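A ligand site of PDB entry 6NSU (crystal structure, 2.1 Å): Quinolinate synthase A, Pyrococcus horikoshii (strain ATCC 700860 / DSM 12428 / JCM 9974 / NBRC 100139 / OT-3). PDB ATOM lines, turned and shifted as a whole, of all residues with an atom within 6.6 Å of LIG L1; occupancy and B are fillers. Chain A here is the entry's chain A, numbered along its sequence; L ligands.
SG of Cys 83 is bound to FE2 of LIG L1 (2.3 Å).
SG of Cys 170 binds FE3 of LIG L1.
ND2 of Asn 111 is in hydrogen-bond range of O2 of LG2 L2 (2.9 Å).
The side-chain sulfur (SG) of Cys 256 binds an iron atom (FE4) of LIG L1, 2.3 Å away.
The side-chain amide nitrogen (ND2) of Asn 111 sits close to a sulfur (S4) of LIG L1.
OH of Tyr 109 sits at hydrogen-bond distance from N1 of LG2 L2.
A ring nitrogen (NE2) of His 21 sits at hydrogen-bond distance from an oxygen (O4) of LG2 L2 (2.9 Å).
O1 of LG2 L2 binds FE1 of LIG L1 (2.0 Å).
The side-chain carboxylate (OE1) of Glu 198 lies close to the side-chain sulfur (SG) of Cys 170.
The backbone NH (N) of Val 172 lies close to the side-chain sulfur (SG) of Cys 170, at 3.4 Å.
N of Gly 258 sits close to SG of Cys 256, 3.5 Å away.
The backbone NH (N) of Tyr 23 lies close to a ring nitrogen (ND1) of His 21 (3.1 Å).
The side-chain sulfur of Cys 83 sits close to the backbone NH of Ala 86 (3.3 Å).
The side-chain carboxylate of Glu 198 sits at hydrogen-bond distance from the side-chain hydroxyl of Tyr 109 (3.1 Å).
The side-chain sulfur (SG) of Cys 170 sits close to a ring nitrogen (ND1) of His 173 (3.2 Å).
The side-chain sulfur of Cys 83 lies close to the backbone NH of Met 85 (3.5 Å).
S4 of LIG L1 lies close to OE1 of Glu 198, at 3.7 Å.
Tyr 23 touches LIG L1 (CE2 to FE1, 3.99 Å).
Hydrophobic or aromatic side chains that line LIG L1: Tyr 23.
Of the 24 residues printed, 6 come within 4 Å of LIG L1.
The nearest printed residue that does not touch LIG L1 is Val 172 (4.04 Å).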
ATOM      1  N   HIS A  21     -15.496   7.637  39.002  1.00  0.00           N
ATOM      2  CA  HIS A  21     -15.279   6.821  37.829  1.00  0.00           C
ATOM      3  C   HIS A  21     -13.973   6.031  37.968  1.00  0.00           C
ATOM      4  O   HIS A  21     -13.087   6.379  38.751  1.00  0.00           O
ATOM      5  CB  HIS A  21     -15.242   7.681  36.565  1.00  0.00           C
ATOM      6  CG  HIS A  21     -15.212   6.897  35.293  1.00  0.00           C
ATOM      7  ND1 HIS A  21     -14.040   6.624  34.615  1.00  0.00           N
ATOM      8  CD2 HIS A  21     -16.207   6.321  34.585  1.00  0.00           C
ATOM      9  CE1 HIS A  21     -14.321   5.912  33.535  1.00  0.00           C
ATOM     10  NE2 HIS A  21     -15.620   5.714  33.489  1.00  0.00           N
ATOM     11  N   TYR A  23     -11.511   5.941  36.181  1.00  0.00           N
ATOM     12  CA  TYR A  23     -10.331   6.705  35.788  1.00  0.00           C
ATOM     13  C   TYR A  23      -9.897   7.711  36.840  1.00  0.00           C
ATOM     14  O   TYR A  23      -8.938   8.462  36.596  1.00  0.00           O
ATOM     15  CB  TYR A  23     -10.597   7.432  34.469  1.00  0.00           C
ATOM     16  CG  TYR A  23     -10.819   6.524  33.274  1.00  0.00           C
ATOM     17  CD1 TYR A  23     -10.538   5.159  33.342  1.00  0.00           C
ATOM     18  CD2 TYR A  23     -11.290   7.035  32.074  1.00  0.00           C
ATOM     19  CE1 TYR A  23     -10.743   4.336  32.248  1.00  0.00           C
ATOM     20  CE2 TYR A  23     -11.491   6.220  30.976  1.00  0.00           C
ATOM     21  CZ  TYR A  23     -11.215   4.873  31.070  1.00  0.00           C
ATOM     22  OH  TYR A  23     -11.420   4.063  29.979  1.00  0.00           O
ATOM     23  N   VAL A  58     -16.244  13.399  34.990  1.00  0.00           N
ATOM     24  CA  VAL A  58     -16.269  14.498  34.029  1.00  0.00           C
ATOM     25  C   VAL A  58     -17.691  15.032  33.908  1.00  0.00           C
ATOM     26  O   VAL A  58     -18.602  14.564  34.597  1.00  0.00           O
ATOM     27  CB  VAL A  58     -15.722  14.054  32.663  1.00  0.00           C
ATOM     28  CG1 VAL A  58     -14.215  13.865  32.738  1.00  0.00           C
ATOM     29  CG2 VAL A  58     -16.385  12.763  32.221  1.00  0.00           C
ATOM     30  N   PHE A  60     -20.223  15.243  31.508  1.00  0.00           N
ATOM     31  CA  PHE A  60     -21.393  14.515  31.018  1.00  0.00           C
ATOM     32  C   PHE A  60     -21.827  13.432  31.996  1.00  0.00           C
ATOM     33  O   PHE A  60     -23.011  13.072  32.042  1.00  0.00           O
ATOM     34  CB  PHE A  60     -21.104  13.910  29.636  1.00  0.00           C
ATOM     35  CG  PHE A  60     -20.258  12.663  29.667  1.00  0.00           C
ATOM     36  CD1 PHE A  60     -20.831  11.415  29.844  1.00  0.00           C
ATOM     37  CD2 PHE A  60     -18.887  12.753  29.495  1.00  0.00           C
ATOM     38  CE1 PHE A  60     -20.056  10.273  29.881  1.00  0.00           C
ATOM     39  CE2 PHE A  60     -18.106  11.607  29.509  1.00  0.00           C
ATOM     40  CZ  PHE A  60     -18.681  10.370  29.706  1.00  0.00           C
ATOM     41  N   MET A  61     -20.889  12.894  32.780  1.00  0.00           N
ATOM     42  CA  MET A  61     -21.238  11.878  33.755  1.00  0.00           C
ATOM     43  C   MET A  61     -22.092  12.468  34.880  1.00  0.00           C
ATOM     44  O   MET A  61     -23.115  11.885  35.276  1.00  0.00           O
ATOM     45  CB  MET A  61     -19.967  11.238  34.313  1.00  0.00           C
ATOM     46  CG  MET A  61     -19.092  10.610  33.254  1.00  0.00           C
ATOM     47  SD  MET A  61     -17.635   9.790  33.941  1.00  0.00           S
ATOM     48  CE  MET A  61     -17.045   8.917  32.482  1.00  0.00           C
ATOM     49  N   THR A  82     -13.890  17.915  32.085  1.00  0.00           N
ATOM     50  CA  THR A  82     -14.706  17.804  30.886  1.00  0.00           C
ATOM     51  C   THR A  82     -14.196  16.668  30.013  1.00  0.00           C
ATOM     52  O   THR A  82     -13.044  16.248  30.102  1.00  0.00           O
ATOM     53  CB  THR A  82     -14.690  19.117  30.078  1.00  0.00           C
ATOM     54  OG1 THR A  82     -13.341  19.426  29.688  1.00  0.00           O
ATOM     55  CG2 THR A  82     -15.238  20.257  30.920  1.00  0.00           C
ATOM     56  N   CYS A  83     -15.085  16.175  29.149  1.00  0.00           N
ATOM     57  CA  CYS A  83     -14.766  15.136  28.175  1.00  0.00           C
ATOM     58  C   CYS A  83     -14.563  15.806  26.822  1.00  0.00           C
ATOM     59  O   CYS A  83     -15.502  16.376  26.254  1.00  0.00           O
ATOM     60  CB  CYS A  83     -15.880  14.093  28.108  1.00  0.00           C
ATOM     61  SG  CYS A  83     -15.729  12.934  26.731  1.00  0.00           S
ATOM     62  N   ALA A  84     -13.334  15.731  26.307  1.00  0.00           N
ATOM     63  CA  ALA A  84     -13.026  16.383  25.044  1.00  0.00           C
ATOM     64  C   ALA A  84     -13.809  15.758  23.885  1.00  0.00           C
ATOM     65  O   ALA A  84     -14.098  16.441  22.897  1.00  0.00           O
ATOM     66  CB  ALA A  84     -11.528  16.314  24.756  1.00  0.00           C
ATOM     67  N   MET A  85     -14.153  14.475  23.994  1.00  0.00           N
ATOM     68  CA  MET A  85     -14.876  13.811  22.913  1.00  0.00           C
ATOM     69  C   MET A  85     -16.342  14.202  22.878  1.00  0.00           C
ATOM     70  O   MET A  85     -16.899  14.421  21.798  1.00  0.00           O
ATOM     71  CB  MET A  85     -14.732  12.296  23.055  1.00  0.00           C
ATOM     72  CG  MET A  85     -15.284  11.523  21.874  1.00  0.00           C
ATOM     73  SD  MET A  85     -15.474   9.775  22.230  1.00  0.00           S
ATOM     74  CE  MET A  85     -17.110   9.761  22.942  1.00  0.00           C
ATOM     75  N   ALA A  86     -16.977  14.295  24.050  1.00  0.00           N
ATOM     76  CA  ALA A  86     -18.394  14.639  24.093  1.00  0.00           C
ATOM     77  C   ALA A  86     -18.642  16.057  23.585  1.00  0.00           C
ATOM     78  O   ALA A  86     -19.699  16.338  23.018  1.00  0.00           O
ATOM     79  CB  ALA A  86     -18.930  14.488  25.514  1.00  0.00           C
ATOM     80  N   TYR A 109     -23.683   7.676  22.097  1.00  0.00           N
ATOM     81  CA  TYR A 109     -22.865   7.241  23.223  1.00  0.00           C
ATOM     82  C   TYR A 109     -23.213   8.052  24.464  1.00  0.00           C
ATOM     83  O   TYR A 109     -23.614   9.216  24.376  1.00  0.00           O
ATOM     84  CB  TYR A 109     -21.386   7.419  22.861  1.00  0.00           C
ATOM     85  CG  TYR A 109     -20.395   6.571  23.617  1.00  0.00           C
ATOM     86  CD1 TYR A 109     -20.815   5.619  24.546  1.00  0.00           C
ATOM     87  CD2 TYR A 109     -19.026   6.717  23.408  1.00  0.00           C
ATOM     88  CE1 TYR A 109     -19.890   4.845  25.234  1.00  0.00           C
ATOM     89  CE2 TYR A 109     -18.104   5.952  24.085  1.00  0.00           C
ATOM     90  CZ  TYR A 109     -18.544   5.023  24.993  1.00  0.00           C
ATOM     91  OH  TYR A 109     -17.623   4.258  25.670  1.00  0.00           O
ATOM     92  N   ASN A 111     -21.161   9.200  26.480  1.00  0.00           N
ATOM     93  CA  ASN A 111     -20.211  10.317  26.456  1.00  0.00           C
ATOM     94  C   ASN A 111     -20.735  11.390  25.510  1.00  0.00           C
ATOM     95  O   ASN A 111     -20.266  11.565  24.387  1.00  0.00           O
ATOM     96  CB  ASN A 111     -18.831   9.823  26.037  1.00  0.00           C
ATOM     97  CG  ASN A 111     -18.336   8.672  26.881  1.00  0.00           C
ATOM     98  OD1 ASN A 111     -19.127   7.888  27.411  1.00  0.00           O
ATOM     99  ND2 ASN A 111     -17.014   8.556  27.021  1.00  0.00           N
ATOM    100  N   HIS A 169     -13.579  11.398  18.353  1.00  0.00           N
ATOM    101  CA  HIS A 169     -12.751  10.352  18.934  1.00  0.00           C
ATOM    102  C   HIS A 169     -12.243  10.818  20.294  1.00  0.00           C
ATOM    103  O   HIS A 169     -12.392  11.989  20.666  1.00  0.00           O
ATOM    104  CB  HIS A 169     -11.573  10.000  18.028  1.00  0.00           C
ATOM    105  CG  HIS A 169     -10.488  11.039  18.018  1.00  0.00           C
ATOM    106  ND1 HIS A 169     -10.559  12.191  17.267  1.00  0.00           N
ATOM    107  CD2 HIS A 169      -9.313  11.095  18.690  1.00  0.00           C
ATOM    108  CE1 HIS A 169      -9.478  12.905  17.463  1.00  0.00           C
ATOM    109  NE2 HIS A 169      -8.699  12.267  18.322  1.00  0.00           N
ATOM    110  N   CYS A 170     -11.642   9.894  21.033  1.00  0.00           N
ATOM    111  CA  CYS A 170     -11.063  10.155  22.342  1.00  0.00           C
ATOM    112  C   CYS A 170      -9.547  10.185  22.205  1.00  0.00           C
ATOM    113  O   CYS A 170      -8.937   9.207  21.760  1.00  0.00           O
ATOM    114  CB  CYS A 170     -11.483   9.096  23.353  1.00  0.00           C
ATOM    115  SG  CYS A 170     -10.418   8.987  24.807  1.00  0.00           S
ATOM    116  N   TYR A 171      -8.932  11.319  22.591  1.00  0.00           N
ATOM    117  CA  TYR A 171      -7.500  11.475  22.416  1.00  0.00           C
ATOM    118  C   TYR A 171      -6.706  10.553  23.349  1.00  0.00           C
ATOM    119  O   TYR A 171      -5.559  10.203  23.032  1.00  0.00           O
ATOM    120  CB  TYR A 171      -7.091  12.930  22.636  1.00  0.00           C
ATOM    121  CG  TYR A 171      -7.222  13.407  24.078  1.00  0.00           C
ATOM    122  CD1 TYR A 171      -8.421  13.919  24.545  1.00  0.00           C
ATOM    123  CD2 TYR A 171      -6.131  13.361  24.940  1.00  0.00           C
ATOM    124  CE1 TYR A 171      -8.540  14.366  25.854  1.00  0.00           C
ATOM    125  CE2 TYR A 171      -6.246  13.802  26.243  1.00  0.00           C
ATOM    126  CZ  TYR A 171      -7.452  14.301  26.702  1.00  0.00           C
ATOM    127  OH  TYR A 171      -7.570  14.737  27.991  1.00  0.00           O
ATOM    128  N   VAL A 172      -7.291  10.153  24.476  1.00  0.00           N
ATOM    129  CA  VAL A 172      -6.587   9.274  25.398  1.00  0.00           C
ATOM    130  C   VAL A 172      -6.405   7.885  24.778  1.00  0.00           C
ATOM    131  O   VAL A 172      -5.286   7.368  24.703  1.00  0.00           O
ATOM    132  CB  VAL A 172      -7.328   9.194  26.748  1.00  0.00           C
ATOM    133  CG1 VAL A 172      -6.586   8.295  27.716  1.00  0.00           C
ATOM    134  CG2 VAL A 172      -7.505  10.583  27.328  1.00  0.00           C
ATOM    135  N   HIS A 173      -7.500   7.288  24.324  1.00  0.00           N
ATOM    136  CA  HIS A 173      -7.428   5.961  23.707  1.00  0.00           C
ATOM    137  C   HIS A 173      -6.851   5.996  22.300  1.00  0.00           C
ATOM    138  O   HIS A 173      -6.437   4.959  21.789  1.00  0.00           O
ATOM    139  CB  HIS A 173      -8.819   5.320  23.686  1.00  0.00           C
ATOM    140  CG  HIS A 173      -9.370   5.015  25.041  1.00  0.00           C
ATOM    141  ND1 HIS A 173     -10.078   5.932  25.781  1.00  0.00           N
ATOM    142  CD2 HIS A 173      -9.287   3.898  25.798  1.00  0.00           C
ATOM    143  CE1 HIS A 173     -10.422   5.381  26.940  1.00  0.00           C
ATOM    144  NE2 HIS A 173      -9.956   4.148  26.968  1.00  0.00           N
ATOM    145  N   GLU A 198     -12.830   2.190  22.393  1.00  0.00           N
ATOM    146  CA  GLU A 198     -12.523   3.529  21.916  1.00  0.00           C
ATOM    147  C   GLU A 198     -11.164   3.622  21.259  1.00  0.00           C
ATOM    148  O   GLU A 198     -10.800   4.698  20.773  1.00  0.00           O
ATOM    149  CB  GLU A 198     -12.622   4.545  23.062  1.00  0.00           C
ATOM    150  CG  GLU A 198     -14.040   4.807  23.549  1.00  0.00           C
ATOM    151  CD  GLU A 198     -14.094   5.880  24.613  1.00  0.00           C
ATOM    152  OE1 GLU A 198     -13.065   6.527  24.866  1.00  0.00           O
ATOM    153  OE2 GLU A 198     -15.178   6.082  25.203  1.00  0.00           O
ATOM    154  N   GLU A 231      -7.245   4.157  29.963  1.00  0.00           N
ATOM    155  CA  GLU A 231      -6.683   5.153  30.869  1.00  0.00           C
ATOM    156  C   GLU A 231      -5.920   4.472  32.001  1.00  0.00           C
ATOM    157  O   GLU A 231      -6.359   3.461  32.556  1.00  0.00           O
ATOM    158  CB  GLU A 231      -7.794   6.038  31.434  1.00  0.00           C
ATOM    159  CG  GLU A 231      -7.409   7.496  31.636  1.00  0.00           C
ATOM    160  CD  GLU A 231      -6.792   7.764  32.994  1.00  0.00           C
ATOM    161  OE1 GLU A 231      -6.661   6.807  33.789  1.00  0.00           O
ATOM    162  OE2 GLU A 231      -6.445   8.931  33.271  1.00  0.00           O
ATOM    163  N   PHE A 255      -3.503   9.234  29.922  1.00  0.00           N
ATOM    164  CA  PHE A 255      -4.265   9.817  31.010  1.00  0.00           C
ATOM    165  C   PHE A 255      -5.250  10.840  30.463  1.00  0.00           C
ATOM    166  O   PHE A 255      -5.016  11.449  29.418  1.00  0.00           O
ATOM    167  CB  PHE A 255      -3.356  10.484  32.049  1.00  0.00           C
ATOM    168  CG  PHE A 255      -2.804  11.795  31.599  1.00  0.00           C
ATOM    169  CD1 PHE A 255      -1.808  11.849  30.635  1.00  0.00           C
ATOM    170  CD2 PHE A 255      -3.270  12.984  32.132  1.00  0.00           C
ATOM    171  CE1 PHE A 255      -1.294  13.061  30.220  1.00  0.00           C
ATOM    172  CE2 PHE A 255      -2.761  14.188  31.721  1.00  0.00           C
ATOM    173  CZ  PHE A 255      -1.768  14.235  30.761  1.00  0.00           C
ATOM    174  N   CYS A 256      -6.354  11.028  31.190  1.00  0.00           N
ATOM    175  CA  CYS A 256      -7.402  11.960  30.807  1.00  0.00           C
ATOM    176  C   CYS A 256      -7.286  13.219  31.664  1.00  0.00           C
ATOM    177  O   CYS A 256      -7.415  13.157  32.887  1.00  0.00           O
ATOM    178  CB  CYS A 256      -8.782  11.328  30.969  1.00  0.00           C
ATOM    179  SG  CYS A 256     -10.148  12.491  30.808  1.00  0.00           S
ATOM    180  N   ILE A 257      -7.047  14.355  31.005  1.00  0.00           N
ATOM    181  CA  ILE A 257      -6.916  15.620  31.730  1.00  0.00           C
ATOM    182  C   ILE A 257      -8.210  15.962  32.458  1.00  0.00           C
ATOM    183  O   ILE A 257      -8.184  16.430  33.603  1.00  0.00           O
ATOM    184  CB  ILE A 257      -6.495  16.751  30.759  1.00  0.00           C
ATOM    185  CG1 ILE A 257      -5.008  16.623  30.396  1.00  0.00           C
ATOM    186  CG2 ILE A 257      -6.775  18.112  31.369  1.00  0.00           C
ATOM    187  CD1 ILE A 257      -4.729  15.699  29.227  1.00  0.00           C
ATOM    188  N   GLY A 258      -9.351  15.715  31.816  1.00  0.00           N
ATOM    189  CA  GLY A 258     -10.623  15.984  32.458  1.00  0.00           C
ATOM    190  C   GLY A 258     -10.808  15.189  33.740  1.00  0.00           C
ATOM    191  O   GLY A 258     -11.322  15.713  34.734  1.00  0.00           O
ATOM    192  N   MET A 259     -10.393  13.925  33.732  1.00  0.00           N
ATOM    193  CA  MET A 259     -10.487  13.110  34.928  1.00  0.00           C
ATOM    194  C   MET A 259      -9.547  13.612  36.020  1.00  0.00           C
ATOM    195  O   MET A 259      -9.902  13.623  37.201  1.00  0.00           O
ATOM    196  CB  MET A 259     -10.190  11.648  34.607  1.00  0.00           C
ATOM    197  CG  MET A 259     -11.318  10.934  33.888  1.00  0.00           C
ATOM    198  SD  MET A 259     -12.800  10.833  34.911  1.00  0.00           S
ATOM    199  CE  MET A 259     -13.891   9.942  33.816  1.00  0.00           C
HETATM  200 FE1  LIG L   1     -13.309   8.992  28.763  1.00  0.00          FE
HETATM  201 FE2  LIG L   1     -13.933  11.742  27.509  1.00  0.00          FE
HETATM  202 FE3  LIG L   1     -11.555  10.075  26.468  1.00  0.00          FE
HETATM  203 FE4  LIG L   1     -11.414  11.380  29.259  1.00  0.00          FE
HETATM  204  S1  LIG L   1     -11.789  12.109  27.220  1.00  0.00           S
HETATM  205  S2  LIG L   1     -11.171   9.349  28.495  1.00  0.00           S
HETATM  206  S3  LIG L   1     -13.554  11.021  29.543  1.00  0.00           S
HETATM  207  S4  LIG L   1     -13.696   9.714  26.722  1.00  0.00           S
HETATM  208  N1  LG2 L   2     -15.846   4.482  28.305  1.00  0.00           N
HETATM  209  C1  LG2 L   2     -15.612   4.570  29.672  1.00  0.00           C
HETATM  210  C2  LG2 L   2     -15.113   5.657  30.296  1.00  0.00           C
HETATM  211  C3  LG2 L   2     -14.787   6.874  29.456  1.00  0.00           C
HETATM  212  O1  LG2 L   2     -14.340   7.855  30.020  1.00  0.00           O
HETATM  213  O2  LG2 L   2     -14.949   6.921  28.243  1.00  0.00           O
HETATM  214  C4  LG2 L   2     -15.931   3.367  30.520  1.00  0.00           C
HETATM  215  O3  LG2 L   2     -16.433   2.257  29.945  1.00  0.00           O
HETATM  216  O4  LG2 L   2     -15.736   3.394  31.718  1.00  0.00           O
